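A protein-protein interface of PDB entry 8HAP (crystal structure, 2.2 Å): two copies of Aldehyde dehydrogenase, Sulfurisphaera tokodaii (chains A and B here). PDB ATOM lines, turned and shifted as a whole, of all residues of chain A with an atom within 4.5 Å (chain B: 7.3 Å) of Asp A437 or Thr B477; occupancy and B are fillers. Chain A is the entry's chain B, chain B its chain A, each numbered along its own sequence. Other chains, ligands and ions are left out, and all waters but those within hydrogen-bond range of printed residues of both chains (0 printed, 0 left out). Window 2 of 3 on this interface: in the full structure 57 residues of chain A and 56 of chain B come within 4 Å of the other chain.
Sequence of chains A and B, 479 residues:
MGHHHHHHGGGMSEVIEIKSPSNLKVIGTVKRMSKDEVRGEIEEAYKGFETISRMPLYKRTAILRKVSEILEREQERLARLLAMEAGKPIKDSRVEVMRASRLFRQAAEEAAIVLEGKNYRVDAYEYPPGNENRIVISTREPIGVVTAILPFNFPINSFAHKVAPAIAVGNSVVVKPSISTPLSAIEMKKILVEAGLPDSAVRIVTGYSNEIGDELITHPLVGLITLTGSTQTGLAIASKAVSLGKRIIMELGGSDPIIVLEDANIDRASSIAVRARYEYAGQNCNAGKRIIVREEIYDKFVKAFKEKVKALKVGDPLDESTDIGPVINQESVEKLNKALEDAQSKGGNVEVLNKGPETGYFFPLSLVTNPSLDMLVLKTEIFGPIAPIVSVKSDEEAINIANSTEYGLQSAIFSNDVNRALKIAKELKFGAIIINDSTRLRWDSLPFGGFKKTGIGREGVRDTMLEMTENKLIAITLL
O of Ile A435 sits at hydrogen-bond distance from N of Thr B477, 3.0 Å away.
OG1 of Thr B477 sits at hydrogen-bond distance from OD2 of Asp A437 (2.7 Å).
The backbone NH (N) of Ile A435 is in hydrogen-bond range of the backbone carbonyl oxygen (O) of Ala B475 (2.6 Å).
The guanidinium group (NH2) of Arg B134 lies within salt-bridge range of the side-chain carboxylate (OD2) of Asp A437 (2.9 Å).
NH1 of Arg A268 sits at hydrogen-bond distance from O of Asn A436 (2.7 Å).
The guanidinium group of Arg A268 is in salt-bridge range of the side-chain carboxylate of Asp A437 (3.7 Å).
NH1 of Arg B134 sits close to O of Gly B130.
O of Ile B135 lies within hydrogen-bond range of N of Ile B476 (2.8 Å).
The guanidinium group (NH1) of Arg B134 is in hydrogen-bond range of the backbone carbonyl oxygen (O) of Pro B129, at 3.0 Å.
OG1 of Thr B477 lies within hydrogen-bond range of NE of Arg B134 (3.3 Å).
Among the printed residues, pairs that only touch across the chains: Arg A268 with Thr B477, Arg A268 with Leu B479, Ile A434 with Ala B475, Ile A435 with Ile B476, Asn A436 with Thr B477, Asn A436 with Leu B479, Leu A441 with Pro B128 and Leu A441 with Arg B134.
Printed residues of chain B within 4 Å of Arg A268: Thr B477 and Leu B479.
Ala A412 touches none of the printed residues of chain B.
Asp A437 touches just these residues of chain B: Arg B134 (2.9 Å) and Thr B477 (2.7 Å).
Of the printed residues of chain A, Arg B134 touches Asp A437 and Leu A441.
Thr B477 touches four residues of chain A.
The nearest printed residue of chain A that does not touch Thr B477 is Leu A441 (4.9 Å).
The nearest printed residue of chain B that does not touch Leu A441 is Thr B477 (4.9 Å).
Hydrophobic or aromatic side chains of chain B within 4 Å of the printed part of chain A: Pro B128, Ala B475 and Leu B479.
Hydrophobic or aromatic side chains of chain A within 4 Å of the printed part of chain B: Ile A434, Ile A435 and Leu A441.
Among the printed residues, Asp or Glu carboxylates within 4 Å of a Lys or Arg side-chain nitrogen of the other chain: Asp A437 with Arg B134 (2.9 Å).
No position is printed for both chains.
Of the 12 pairs that touch across the chains among the printed residues, none has its exchanged pair printed and touching as well.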
ATOM      1  N   ARG A 268      -7.220 -35.598  -4.431  1.00  0.00           N
ATOM      2  CA  ARG A 268      -6.789 -34.672  -5.501  1.00  0.00           C
ATOM      3  C   ARG A 268      -6.209 -35.454  -6.696  1.00  0.00           C
ATOM      4  O   ARG A 268      -6.598 -35.146  -7.850  1.00  0.00           O
ATOM      5  CB  ARG A 268      -5.769 -33.683  -4.938  1.00  0.00           C
ATOM      6  CG  ARG A 268      -5.428 -32.566  -5.909  1.00  0.00           C
ATOM      7  CD  ARG A 268      -5.361 -31.185  -5.285  1.00  0.00           C
ATOM      8  NE  ARG A 268      -5.080 -30.196  -6.328  1.00  0.00           N
ATOM      9  CZ  ARG A 268      -3.928 -30.101  -6.976  1.00  0.00           C
ATOM     10  NH1 ARG A 268      -2.943 -30.935  -6.692  1.00  0.00           N
ATOM     11  NH2 ARG A 268      -3.764 -29.185  -7.913  1.00  0.00           N
ATOM     12  N   ILE A 272      -8.153 -35.430 -10.448  1.00  0.00           N
ATOM     13  CA  ILE A 272      -7.408 -34.858 -11.603  1.00  0.00           C
ATOM     14  C   ILE A 272      -7.102 -35.991 -12.590  1.00  0.00           C
ATOM     15  O   ILE A 272      -7.208 -35.750 -13.796  1.00  0.00           O
ATOM     16  CB  ILE A 272      -6.140 -34.125 -11.131  1.00  0.00           C
ATOM     17  CG1 ILE A 272      -6.482 -32.855 -10.338  1.00  0.00           C
ATOM     18  CG2 ILE A 272      -5.210 -33.831 -12.299  1.00  0.00           C
ATOM     19  CD1 ILE A 272      -5.267 -32.098  -9.807  1.00  0.00           C
ATOM     20  N   ALA A 412       2.879 -36.093 -15.319  1.00  0.00           N
ATOM     21  CA  ALA A 412       2.569 -35.502 -13.998  1.00  0.00           C
ATOM     22  C   ALA A 412       3.055 -36.406 -12.859  1.00  0.00           C
ATOM     23  O   ALA A 412       3.129 -37.651 -13.034  1.00  0.00           O
ATOM     24  CB  ALA A 412       1.096 -35.217 -13.879  1.00  0.00           C
ATOM     25  N   PHE A 414       2.221 -36.686  -8.663  1.00  0.00           N
ATOM     26  CA  PHE A 414       1.502 -36.359  -7.416  1.00  0.00           C
ATOM     27  C   PHE A 414       2.345 -36.885  -6.248  1.00  0.00           C
ATOM     28  O   PHE A 414       2.817 -38.059  -6.279  1.00  0.00           O
ATOM     29  CB  PHE A 414       0.084 -36.906  -7.487  1.00  0.00           C
ATOM     30  CG  PHE A 414      -0.767 -36.142  -8.464  1.00  0.00           C
ATOM     31  CD1 PHE A 414      -0.797 -36.491  -9.807  1.00  0.00           C
ATOM     32  CD2 PHE A 414      -1.478 -35.031  -8.047  1.00  0.00           C
ATOM     33  CE1 PHE A 414      -1.561 -35.766 -10.706  1.00  0.00           C
ATOM     34  CE2 PHE A 414      -2.246 -34.308  -8.946  1.00  0.00           C
ATOM     35  CZ  PHE A 414      -2.294 -34.679 -10.271  1.00  0.00           C
ATOM     36  N   ILE A 434       4.607 -32.022 -14.876  1.00  0.00           N
ATOM     37  CA  ILE A 434       3.635 -31.259 -14.050  1.00  0.00           C
ATOM     38  C   ILE A 434       3.632 -31.819 -12.628  1.00  0.00           C
ATOM     39  O   ILE A 434       3.284 -32.980 -12.445  1.00  0.00           O
ATOM     40  CB  ILE A 434       2.226 -31.301 -14.669  1.00  0.00           C
ATOM     41  CG1 ILE A 434       2.246 -30.984 -16.168  1.00  0.00           C
ATOM     42  CG2 ILE A 434       1.312 -30.369 -13.895  1.00  0.00           C
ATOM     43  CD1 ILE A 434       2.722 -29.592 -16.517  1.00  0.00           C
ATOM     44  N   ILE A 435       4.036 -31.016 -11.653  1.00  0.00           N
ATOM     45  CA  ILE A 435       4.124 -31.498 -10.261  1.00  0.00           C
ATOM     46  C   ILE A 435       2.870 -31.041  -9.542  1.00  0.00           C
ATOM     47  O   ILE A 435       2.642 -29.805  -9.447  1.00  0.00           O
ATOM     48  CB  ILE A 435       5.414 -31.048  -9.564  1.00  0.00           C
ATOM     49  CG1 ILE A 435       6.626 -31.651 -10.268  1.00  0.00           C
ATOM     50  CG2 ILE A 435       5.343 -31.429  -8.090  1.00  0.00           C
ATOM     51  CD1 ILE A 435       7.939 -31.166  -9.724  1.00  0.00           C
ATOM     52  N   ASN A 436       2.111 -32.039  -9.081  1.00  0.00           N
ATOM     53  CA  ASN A 436       0.840 -31.913  -8.355  1.00  0.00           C
ATOM     54  C   ASN A 436      -0.248 -31.293  -9.222  1.00  0.00           C
ATOM     55  O   ASN A 436      -1.152 -30.668  -8.640  1.00  0.00           O
ATOM     56  CB  ASN A 436       1.094 -31.215  -7.034  1.00  0.00           C
ATOM     57  CG  ASN A 436       1.724 -32.209  -6.085  1.00  0.00           C
ATOM     58  OD1 ASN A 436       1.392 -33.394  -6.144  1.00  0.00           O
ATOM     59  ND2 ASN A 436       2.688 -31.767  -5.296  1.00  0.00           N
ATOM     60  N   ASP A 437      -0.242 -31.528 -10.530  1.00  0.00           N
ATOM     61  CA  ASP A 437      -1.375 -31.071 -11.380  1.00  0.00           C
ATOM     62  C   ASP A 437      -1.526 -31.969 -12.608  1.00  0.00           C
ATOM     63  O   ASP A 437      -0.754 -32.935 -12.749  1.00  0.00           O
ATOM     64  CB  ASP A 437      -1.216 -29.586 -11.748  1.00  0.00           C
ATOM     65  CG  ASP A 437      -2.519 -28.806 -11.717  1.00  0.00           C
ATOM     66  OD1 ASP A 437      -3.522 -29.313 -12.284  1.00  0.00           O
ATOM     67  OD2 ASP A 437      -2.521 -27.690 -11.117  1.00  0.00           O
ATOM     68  N   SER A 438      -2.486 -31.630 -13.481  1.00  0.00           N
ATOM     69  CA  SER A 438      -2.892 -32.442 -14.649  1.00  0.00           C
ATOM     70  C   SER A 438      -1.849 -32.422 -15.773  1.00  0.00           C
ATOM     71  O   SER A 438      -1.272 -31.361 -16.033  1.00  0.00           O
ATOM     72  CB  SER A 438      -4.189 -31.949 -15.156  1.00  0.00           C
ATOM     73  OG  SER A 438      -4.515 -32.648 -16.325  1.00  0.00           O
ATOM     74  N   THR A 439      -1.717 -33.539 -16.500  1.00  0.00           N
ATOM     75  CA  THR A 439      -1.029 -33.634 -17.818  1.00  0.00           C
ATOM     76  C   THR A 439      -1.703 -32.699 -18.852  1.00  0.00           C
ATOM     77  O   THR A 439      -1.039 -32.309 -19.825  1.00  0.00           O
ATOM     78  CB  THR A 439      -1.025 -35.067 -18.385  1.00  0.00           C
ATOM     79  OG1 THR A 439      -2.349 -35.597 -18.405  1.00  0.00           O
ATOM     80  CG2 THR A 439      -0.141 -36.002 -17.616  1.00  0.00           C
ATOM     81  N   LEU A 441      -2.459 -29.550 -18.636  1.00  0.00           N
ATOM     82  CA  LEU A 441      -2.064 -28.121 -18.590  1.00  0.00           C
ATOM     83  C   LEU A 441      -1.294 -27.727 -19.858  1.00  0.00           C
ATOM     84  O   LEU A 441      -0.411 -28.473 -20.335  1.00  0.00           O
ATOM     85  CB  LEU A 441      -1.218 -27.835 -17.357  1.00  0.00           C
ATOM     86  CG  LEU A 441      -1.868 -28.065 -16.006  1.00  0.00           C
ATOM     87  CD1 LEU A 441      -1.063 -27.345 -14.946  1.00  0.00           C
ATOM     88  CD2 LEU A 441      -3.329 -27.648 -15.992  1.00  0.00           C
ATOM     89  N   PRO B 128      -4.306 -22.129 -17.887  1.00  0.00           N
ATOM     90  CA  PRO B 128      -5.351 -22.792 -17.109  1.00  0.00           C
ATOM     91  C   PRO B 128      -5.641 -21.973 -15.860  1.00  0.00           C
ATOM     92  O   PRO B 128      -4.801 -21.170 -15.445  1.00  0.00           O
ATOM     93  CB  PRO B 128      -4.734 -24.156 -16.762  1.00  0.00           C
ATOM     94  CG  PRO B 128      -3.667 -24.357 -17.820  1.00  0.00           C
ATOM     95  CD  PRO B 128      -3.112 -22.971 -18.023  1.00  0.00           C
ATOM     96  N   PRO B 129      -6.830 -22.136 -15.229  1.00  0.00           N
ATOM     97  CA  PRO B 129      -7.130 -21.422 -13.984  1.00  0.00           C
ATOM     98  C   PRO B 129      -6.153 -21.823 -12.866  1.00  0.00           C
ATOM     99  O   PRO B 129      -5.712 -22.928 -12.876  1.00  0.00           O
ATOM    100  CB  PRO B 129      -8.591 -21.786 -13.642  1.00  0.00           C
ATOM    101  CG  PRO B 129      -8.988 -22.908 -14.601  1.00  0.00           C
ATOM    102  CD  PRO B 129      -7.962 -22.933 -15.720  1.00  0.00           C
ATOM    103  N   GLY B 130      -5.792 -20.896 -11.970  1.00  0.00           N
ATOM    104  CA  GLY B 130      -4.913 -21.169 -10.813  1.00  0.00           C
ATOM    105  C   GLY B 130      -3.432 -20.928 -11.084  1.00  0.00           C
ATOM    106  O   GLY B 130      -2.604 -21.329 -10.258  1.00  0.00           O
ATOM    107  N   ASN B 133      -0.837 -19.799  -8.385  1.00  0.00           N
ATOM    108  CA  ASN B 133      -0.281 -20.780  -7.411  1.00  0.00           C
ATOM    109  C   ASN B 133       0.775 -21.663  -8.083  1.00  0.00           C
ATOM    110  O   ASN B 133       1.139 -22.673  -7.476  1.00  0.00           O
ATOM    111  CB  ASN B 133      -1.371 -21.679  -6.814  1.00  0.00           C
ATOM    112  CG  ASN B 133      -2.416 -20.873  -6.084  1.00  0.00           C
ATOM    113  OD1 ASN B 133      -2.088 -20.055  -5.216  1.00  0.00           O
ATOM    114  ND2 ASN B 133      -3.665 -21.042  -6.484  1.00  0.00           N
ATOM    115  N   ARG B 134       1.238 -21.302  -9.286  1.00  0.00           N
ATOM    116  CA  ARG B 134       2.187 -22.139 -10.065  1.00  0.00           C
ATOM    117  C   ARG B 134       3.565 -21.486 -10.193  1.00  0.00           C
ATOM    118  O   ARG B 134       3.675 -20.268 -10.318  1.00  0.00           O
ATOM    119  CB  ARG B 134       1.639 -22.470 -11.454  1.00  0.00           C
ATOM    120  CG  ARG B 134       0.395 -23.338 -11.430  1.00  0.00           C
ATOM    121  CD  ARG B 134       0.010 -23.889 -12.780  1.00  0.00           C
ATOM    122  NE  ARG B 134      -1.143 -24.752 -12.593  1.00  0.00           N
ATOM    123  CZ  ARG B 134      -2.414 -24.397 -12.765  1.00  0.00           C
ATOM    124  NH1 ARG B 134      -2.741 -23.188 -13.199  1.00  0.00           N
ATOM    125  NH2 ARG B 134      -3.372 -25.271 -12.508  1.00  0.00           N
ATOM    126  N   ILE B 135       4.597 -22.320 -10.155  1.00  0.00           N
ATOM    127  CA  ILE B 135       5.954 -21.996 -10.651  1.00  0.00           C
ATOM    128  C   ILE B 135       6.146 -22.810 -11.920  1.00  0.00           C
ATOM    129  O   ILE B 135       6.031 -24.067 -11.853  1.00  0.00           O
ATOM    130  CB  ILE B 135       7.026 -22.292  -9.581  1.00  0.00           C
ATOM    131  CG1 ILE B 135       6.755 -21.473  -8.319  1.00  0.00           C
ATOM    132  CG2 ILE B 135       8.402 -22.024 -10.157  1.00  0.00           C
ATOM    133  CD1 ILE B 135       7.557 -21.869  -7.113  1.00  0.00           C
ATOM    134  N   VAL B 136       6.460 -22.134 -13.025  1.00  0.00           N
ATOM    135  CA  VAL B 136       6.777 -22.831 -14.293  1.00  0.00           C
ATOM    136  C   VAL B 136       8.156 -22.378 -14.767  1.00  0.00           C
ATOM    137  O   VAL B 136       8.343 -21.156 -15.064  1.00  0.00           O
ATOM    138  CB  VAL B 136       5.655 -22.589 -15.317  1.00  0.00           C
ATOM    139  CG1 VAL B 136       5.766 -23.502 -16.503  1.00  0.00           C
ATOM    140  CG2 VAL B 136       4.295 -22.742 -14.657  1.00  0.00           C
ATOM    141  N   ALA B 475       6.382 -27.546 -14.285  1.00  0.00           N
ATOM    142  CA  ALA B 475       5.293 -26.799 -13.614  1.00  0.00           C
ATOM    143  C   ALA B 475       4.978 -27.420 -12.248  1.00  0.00           C
ATOM    144  O   ALA B 475       4.484 -28.556 -12.223  1.00  0.00           O
ATOM    145  CB  ALA B 475       4.062 -26.785 -14.481  1.00  0.00           C
ATOM    146  N   ILE B 476       5.182 -26.636 -11.183  1.00  0.00           N
ATOM    147  CA  ILE B 476       4.804 -26.932  -9.783  1.00  0.00           C
ATOM    148  C   ILE B 476       3.535 -26.140  -9.438  1.00  0.00           C
ATOM    149  O   ILE B 476       3.538 -24.908  -9.578  1.00  0.00           O
ATOM    150  CB  ILE B 476       5.939 -26.577  -8.800  1.00  0.00           C
ATOM    151  CG1 ILE B 476       7.292 -27.143  -9.225  1.00  0.00           C
ATOM    152  CG2 ILE B 476       5.569 -27.044  -7.403  1.00  0.00           C
ATOM    153  CD1 ILE B 476       8.471 -26.378  -8.665  1.00  0.00           C
ATOM    154  N   THR B 477       2.474 -26.833  -9.021  1.00  0.00           N
ATOM    155  CA  THR B 477       1.295 -26.232  -8.368  1.00  0.00           C
ATOM    156  C   THR B 477       1.557 -26.315  -6.870  1.00  0.00           C
ATOM    157  O   THR B 477       1.562 -27.452  -6.394  1.00  0.00           O
ATOM    158  CB  THR B 477      -0.010 -26.933  -8.772  1.00  0.00           C
ATOM    159  OG1 THR B 477      -0.159 -26.810 -10.186  1.00  0.00           O
ATOM    160  CG2 THR B 477      -1.240 -26.329  -8.126  1.00  0.00           C
ATOM    161  N   LEU B 478       1.824 -25.172  -6.213  1.00  0.00           N
ATOM    162  CA  LEU B 478       1.985 -25.015  -4.742  1.00  0.00           C
ATOM    163  C   LEU B 478       0.661 -25.396  -4.062  1.00  0.00           C
ATOM    164  O   LEU B 478      -0.366 -24.891  -4.487  1.00  0.00           O
ATOM    165  CB  LEU B 478       2.332 -23.554  -4.433  1.00  0.00           C
ATOM    166  CG  LEU B 478       3.811 -23.154  -4.379  1.00  0.00           C
ATOM    167  CD1 LEU B 478       4.766 -24.291  -4.708  1.00  0.00           C
ATOM    168  CD2 LEU B 478       4.087 -21.945  -5.260  1.00  0.00           C
ATOM    169  N   LEU B 479       0.691 -26.235  -3.030  1.00  0.00           N
ATOM    170  CA  LEU B 479      -0.530 -26.855  -2.426  1.00  0.00           C
ATOM    171  C   LEU B 479      -0.813 -26.220  -1.057  1.00  0.00           C
ATOM    172  O   LEU B 479       0.149 -25.816  -0.400  1.00  0.00           O
ATOM    173  CB  LEU B 479      -0.314 -28.374  -2.326  1.00  0.00           C
ATOM    174  CG  LEU B 479      -1.061 -29.267  -3.321  1.00  0.00           C
ATOM    175  CD1 LEU B 479      -1.634 -28.490  -4.504  1.00  0.00           C
ATOM    176  CD2 LEU B 479      -0.162 -30.407  -3.794  1.00  0.00           C
